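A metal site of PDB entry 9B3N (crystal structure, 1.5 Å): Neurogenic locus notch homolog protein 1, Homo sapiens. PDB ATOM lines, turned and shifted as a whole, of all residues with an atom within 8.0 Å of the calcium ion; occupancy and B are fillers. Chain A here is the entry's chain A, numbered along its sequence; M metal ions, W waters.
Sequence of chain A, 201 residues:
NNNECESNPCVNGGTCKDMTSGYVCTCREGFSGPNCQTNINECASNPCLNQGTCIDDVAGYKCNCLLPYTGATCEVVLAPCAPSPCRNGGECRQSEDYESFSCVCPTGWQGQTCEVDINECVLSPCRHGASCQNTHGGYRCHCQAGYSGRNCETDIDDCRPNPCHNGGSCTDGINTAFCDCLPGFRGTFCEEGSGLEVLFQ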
ATOM      1  N   THR A 107     -17.647 -25.930  -8.067  1.00  0.00           N
ATOM      2  CA  THR A 107     -16.199 -25.914  -8.015  1.00  0.00           C
ATOM      3  C   THR A 107     -15.771 -25.967  -6.556  1.00  0.00           C
ATOM      4  O   THR A 107     -16.377 -25.346  -5.678  1.00  0.00           O
ATOM      5  CB  THR A 107     -15.637 -24.650  -8.702  1.00  0.00           C
ATOM      6  OG1 THR A 107     -16.268 -24.531  -9.976  1.00  0.00           O
ATOM      7  CG2 THR A 107     -14.168 -24.779  -8.905  1.00  0.00           C
ATOM      8  N   GLY A 108     -14.782 -26.770  -6.286  1.00  0.00           N
ATOM      9  CA  GLY A 108     -14.232 -26.817  -4.977  1.00  0.00           C
ATOM     10  C   GLY A 108     -14.719 -27.972  -4.136  1.00  0.00           C
ATOM     11  O   GLY A 108     -14.139 -28.205  -3.076  1.00  0.00           O
ATOM     12  N   TRP A 109     -15.815 -28.627  -4.543  1.00  0.00           N
ATOM     13  CA  TRP A 109     -16.407 -29.696  -3.769  1.00  0.00           C
ATOM     14  C   TRP A 109     -16.529 -30.967  -4.608  1.00  0.00           C
ATOM     15  O   TRP A 109     -16.596 -30.908  -5.835  1.00  0.00           O
ATOM     16  CB  TRP A 109     -17.808 -29.316  -3.280  1.00  0.00           C
ATOM     17  CG  TRP A 109     -17.778 -28.200  -2.286  1.00  0.00           C
ATOM     18  CD1 TRP A 109     -18.103 -26.889  -2.492  1.00  0.00           C
ATOM     19  CD2 TRP A 109     -17.442 -28.328  -0.903  1.00  0.00           C
ATOM     20  NE1 TRP A 109     -18.003 -26.200  -1.312  1.00  0.00           N
ATOM     21  CE2 TRP A 109     -17.594 -27.054  -0.322  1.00  0.00           C
ATOM     22  CE3 TRP A 109     -17.051 -29.415  -0.088  1.00  0.00           C
ATOM     23  CZ2 TRP A 109     -17.353 -26.836   1.039  1.00  0.00           C
ATOM     24  CZ3 TRP A 109     -16.812 -29.196   1.250  1.00  0.00           C
ATOM     25  CH2 TRP A 109     -16.948 -27.909   1.799  1.00  0.00           C
ATOM     26  N   VAL A 116     -17.223 -33.255   0.319  1.00  0.00           N
ATOM     27  CA  VAL A 116     -15.800 -33.478   0.487  1.00  0.00           C
ATOM     28  C   VAL A 116     -15.043 -32.378  -0.232  1.00  0.00           C
ATOM     29  O   VAL A 116     -15.252 -32.151  -1.434  1.00  0.00           O
ATOM     30  CB  VAL A 116     -15.410 -34.856  -0.058  1.00  0.00           C
ATOM     31  CG1 VAL A 116     -13.946 -35.044   0.086  1.00  0.00           C
ATOM     32  CG2 VAL A 116     -16.212 -35.958   0.663  1.00  0.00           C
ATOM     33  N   ASP A 117     -14.121 -31.763   0.469  1.00  0.00           N
ATOM     34  CA  ASP A 117     -13.317 -30.707  -0.116  1.00  0.00           C
ATOM     35  C   ASP A 117     -12.447 -31.255  -1.248  1.00  0.00           C
ATOM     36  O   ASP A 117     -12.071 -32.450  -1.276  1.00  0.00           O
ATOM     37  CB  ASP A 117     -12.427 -30.083   0.960  1.00  0.00           C
ATOM     38  CG  ASP A 117     -11.562 -28.934   0.399  1.00  0.00           C
ATOM     39  OD1 ASP A 117     -12.124 -28.038  -0.263  1.00  0.00           O
ATOM     40  OD2 ASP A 117     -10.339 -29.030   0.543  1.00  0.00           O
ATOM     41  N   ILE A 118     -12.125 -30.357  -2.204  1.00  0.00           N
ATOM     42  CA  ILE A 118     -11.073 -30.608  -3.183  1.00  0.00           C
ATOM     43  C   ILE A 118      -9.852 -29.837  -2.719  1.00  0.00           C
ATOM     44  O   ILE A 118      -9.983 -28.667  -2.427  1.00  0.00           O
ATOM     45  CB  ILE A 118     -11.465 -30.113  -4.578  1.00  0.00           C
ATOM     46  CG1 ILE A 118     -12.517 -31.097  -5.151  1.00  0.00           C
ATOM     47  CG2 ILE A 118     -10.248 -30.101  -5.544  1.00  0.00           C
ATOM     48  CD1 ILE A 118     -13.197 -30.667  -6.474  1.00  0.00           C
ATOM     49  N   ASN A 119      -8.690 -30.465  -2.660  1.00  0.00           N
ATOM     50  CA  ASN A 119      -7.508 -29.694  -2.243  1.00  0.00           C
ATOM     51  C   ASN A 119      -6.828 -29.146  -3.487  1.00  0.00           C
ATOM     52  O   ASN A 119      -6.076 -29.837  -4.162  1.00  0.00           O
ATOM     53  CB  ASN A 119      -6.590 -30.524  -1.369  1.00  0.00           C
ATOM     54  CG  ASN A 119      -5.449 -29.713  -0.814  1.00  0.00           C
ATOM     55  OD1 ASN A 119      -5.108 -28.675  -1.343  1.00  0.00           O
ATOM     56  ND2 ASN A 119      -4.794 -30.249   0.201  1.00  0.00           N
ATOM     57  N   GLU A 120      -7.086 -27.865  -3.766  1.00  0.00           N
ATOM     58  CA  GLU A 120      -6.483 -27.197  -4.919  1.00  0.00           C
ATOM     59  C   GLU A 120      -4.974 -27.059  -4.797  1.00  0.00           C
ATOM     60  O   GLU A 120      -4.306 -26.895  -5.807  1.00  0.00           O
ATOM     61  CB  GLU A 120      -7.131 -25.820  -5.113  1.00  0.00           C
ATOM     62  CG  GLU A 120      -8.595 -25.965  -5.606  1.00  0.00           C
ATOM     63  CD  GLU A 120      -9.614 -25.991  -4.475  1.00  0.00           C
ATOM     64  OE1 GLU A 120      -9.191 -26.050  -3.313  1.00  0.00           O
ATOM     65  OE2 GLU A 120     -10.820 -25.806  -4.777  1.00  0.00           O
ATOM     66  N   CYS A 121      -4.424 -27.170  -3.603  1.00  0.00           N
ATOM     67  CA  CYS A 121      -2.992 -26.948  -3.460  1.00  0.00           C
ATOM     68  C   CYS A 121      -2.181 -28.161  -3.863  1.00  0.00           C
ATOM     69  O   CYS A 121      -0.958 -28.050  -4.027  1.00  0.00           O
ATOM     70  CB  CYS A 121      -2.695 -26.559  -2.027  1.00  0.00           C
ATOM     71  SG  CYS A 121      -3.519 -25.056  -1.614  1.00  0.00           S
ATOM     72  N   GLN A 133      -2.943 -22.001   0.134  1.00  0.00           N
ATOM     73  CA  GLN A 133      -3.600 -22.396   1.366  1.00  0.00           C
ATOM     74  C   GLN A 133      -4.901 -23.057   0.983  1.00  0.00           C
ATOM     75  O   GLN A 133      -5.755 -22.426   0.347  1.00  0.00           O
ATOM     76  CB  GLN A 133      -3.879 -21.178   2.260  1.00  0.00           C
ATOM     77  CG  GLN A 133      -4.697 -21.595   3.468  1.00  0.00           C
ATOM     78  CD  GLN A 133      -5.192 -20.420   4.301  1.00  0.00           C
ATOM     79  OE1 GLN A 133      -4.978 -19.261   3.937  1.00  0.00           O
ATOM     80  NE2 GLN A 133      -5.885 -20.721   5.404  1.00  0.00           N
ATOM     81  N   ASN A 134      -5.050 -24.321   1.321  1.00  0.00           N
ATOM     82  CA  ASN A 134      -6.319 -25.004   1.011  1.00  0.00           C
ATOM     83  C   ASN A 134      -7.337 -24.624   2.076  1.00  0.00           C
ATOM     84  O   ASN A 134      -6.993 -24.469   3.262  1.00  0.00           O
ATOM     85  CB  ASN A 134      -6.158 -26.506   0.975  1.00  0.00           C
ATOM     86  CG  ASN A 134      -7.431 -27.194   0.576  1.00  0.00           C
ATOM     87  OD1 ASN A 134      -8.071 -26.742  -0.367  1.00  0.00           O
ATOM     88  ND2 ASN A 134      -7.830 -28.227   1.311  1.00  0.00           N
ATOM     89  N   THR A 135      -8.566 -24.395   1.661  1.00  0.00           N
ATOM     90  CA  THR A 135      -9.700 -24.205   2.547  1.00  0.00           C
ATOM     91  C   THR A 135     -10.835 -25.187   2.194  1.00  0.00           C
ATOM     92  O   THR A 135     -10.863 -25.806   1.135  1.00  0.00           O
ATOM     93  CB  THR A 135     -10.234 -22.756   2.485  1.00  0.00           C
ATOM     94  OG1 THR A 135     -10.991 -22.580   1.283  1.00  0.00           O
ATOM     95  CG2 THR A 135      -9.098 -21.661   2.574  1.00  0.00           C
ATOM     96  N   HIS A 136     -11.807 -25.277   3.090  1.00  0.00           N
ATOM     97  CA  HIS A 136     -12.987 -26.118   2.867  1.00  0.00           C
ATOM     98  C   HIS A 136     -13.885 -25.488   1.807  1.00  0.00           C
ATOM     99  O   HIS A 136     -14.574 -24.490   2.081  1.00  0.00           O
ATOM    100  CB  HIS A 136     -13.726 -26.343   4.170  1.00  0.00           C
ATOM    101  CG  HIS A 136     -13.103 -27.384   5.014  1.00  0.00           C
ATOM    102  ND1 HIS A 136     -13.453 -28.711   4.924  1.00  0.00           N
ATOM    103  CD2 HIS A 136     -12.136 -27.310   5.961  1.00  0.00           C
ATOM    104  CE1 HIS A 136     -12.738 -29.415   5.789  1.00  0.00           C
ATOM    105  NE2 HIS A 136     -11.922 -28.583   6.426  1.00  0.00           N
ATOM    106  N   GLY A 137     -13.799 -25.991   0.604  1.00  0.00           N
ATOM    107  CA  GLY A 137     -14.571 -25.529  -0.529  1.00  0.00           C
ATOM    108  C   GLY A 137     -13.907 -24.413  -1.310  1.00  0.00           C
ATOM    109  O   GLY A 137     -14.475 -23.942  -2.306  1.00  0.00           O
ATOM    110  N   GLY A 138     -12.702 -24.020  -0.944  1.00  0.00           N
ATOM    111  CA  GLY A 138     -11.907 -23.132  -1.778  1.00  0.00           C
ATOM    112  C   GLY A 138     -10.433 -23.265  -1.524  1.00  0.00           C
ATOM    113  O   GLY A 138      -9.943 -24.342  -1.145  1.00  0.00           O
ATOM    114  N   TYR A 139      -9.738 -22.163  -1.805  1.00  0.00           N
ATOM    115  CA  TYR A 139      -8.324 -22.041  -1.526  1.00  0.00           C
ATOM    116  C   TYR A 139      -8.001 -20.577  -1.581  1.00  0.00           C
ATOM    117  O   TYR A 139      -8.826 -19.756  -1.967  1.00  0.00           O
ATOM    118  CB  TYR A 139      -7.432 -22.774  -2.533  1.00  0.00           C
ATOM    119  CG  TYR A 139      -7.446 -22.190  -3.935  1.00  0.00           C
ATOM    120  CD1 TYR A 139      -8.476 -22.452  -4.824  1.00  0.00           C
ATOM    121  CD2 TYR A 139      -6.413 -21.366  -4.364  1.00  0.00           C
ATOM    122  CE1 TYR A 139      -8.482 -21.893  -6.115  1.00  0.00           C
ATOM    123  CE2 TYR A 139      -6.411 -20.838  -5.626  1.00  0.00           C
ATOM    124  CZ  TYR A 139      -7.430 -21.061  -6.487  1.00  0.00           C
ATOM    125  OH  TYR A 139      -7.437 -20.514  -7.742  1.00  0.00           O
ATOM    126  N   ARG A 140      -6.771 -20.273  -1.207  1.00  0.00           N
ATOM    127  CA  ARG A 140      -6.308 -18.901  -1.215  1.00  0.00           C
ATOM    128  C   ARG A 140      -4.833 -18.941  -1.593  1.00  0.00           C
ATOM    129  O   ARG A 140      -4.099 -19.804  -1.110  1.00  0.00           O
ATOM    130  CB  ARG A 140      -6.495 -18.264   0.162  1.00  0.00           C
ATOM    131  CG  ARG A 140      -5.891 -16.904   0.360  1.00  0.00           C
ATOM    132  CD  ARG A 140      -6.580 -15.743  -0.354  1.00  0.00           C
ATOM    133  NE  ARG A 140      -5.872 -14.513   0.003  1.00  0.00           N
ATOM    134  CZ  ARG A 140      -6.208 -13.749   1.040  1.00  0.00           C
ATOM    135  NH1 ARG A 140      -7.213 -14.089   1.850  1.00  0.00           N
ATOM    136  NH2 ARG A 140      -5.533 -12.594   1.243  1.00  0.00           N
HETATM  137 CA    CA M   1     -10.347 -26.683  -1.133  1.00  0.00          CA
HETATM  138  O   HOH W   1     -12.188 -26.356  -2.568  1.00  0.00           O
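The side-chain hydroxyl of Thr 135 sits close to the backbone NH of Gly 138, 3.2 Å away. The backbone carbonyl oxygen (O) of Gly 108 lies within hydrogen-bond range of the backbone NH (N) of Ile 118 (3.1 Å). The side-chain carboxylate (OD1) of Asp 117 sits close to the backbone NH (N) of Gly 137. The backbone NH of Asn 134 lies within hydrogen-bond range of the side-chain sulfur of Cys 121, at 3.4 Å. The side-chain hydroxyl (OG1) of Thr 135 is in hydrogen-bond range of the backbone NH (N) of Tyr 139.
The calcium ion is bound by water W1 (2.4 Å), O of Gly 138 (2.4 Å), O of Ile 118 (2.4 Å), OD1 of Asp 117 (2.4 Å), OD1 of Asn 134 (2.4 Å), O of Thr 135 (2.5 Å), OE1 of Glu 120 (2.5 Å) and OD2 of Asp 117 (2.9 Å). The calcium ion has eight donor atoms within binding distance.
Gly 137 touches the calcium ion (N to CA, 3.9 Å). Of the 17 residues printed, 7 come within 4 Å of the calcium ion. Along chain A the residues within 4 Å of the calcium ion span positions 117 to 138. The nearest printed residue that does not touch the calcium ion is Asn 119 (4.3 Å).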
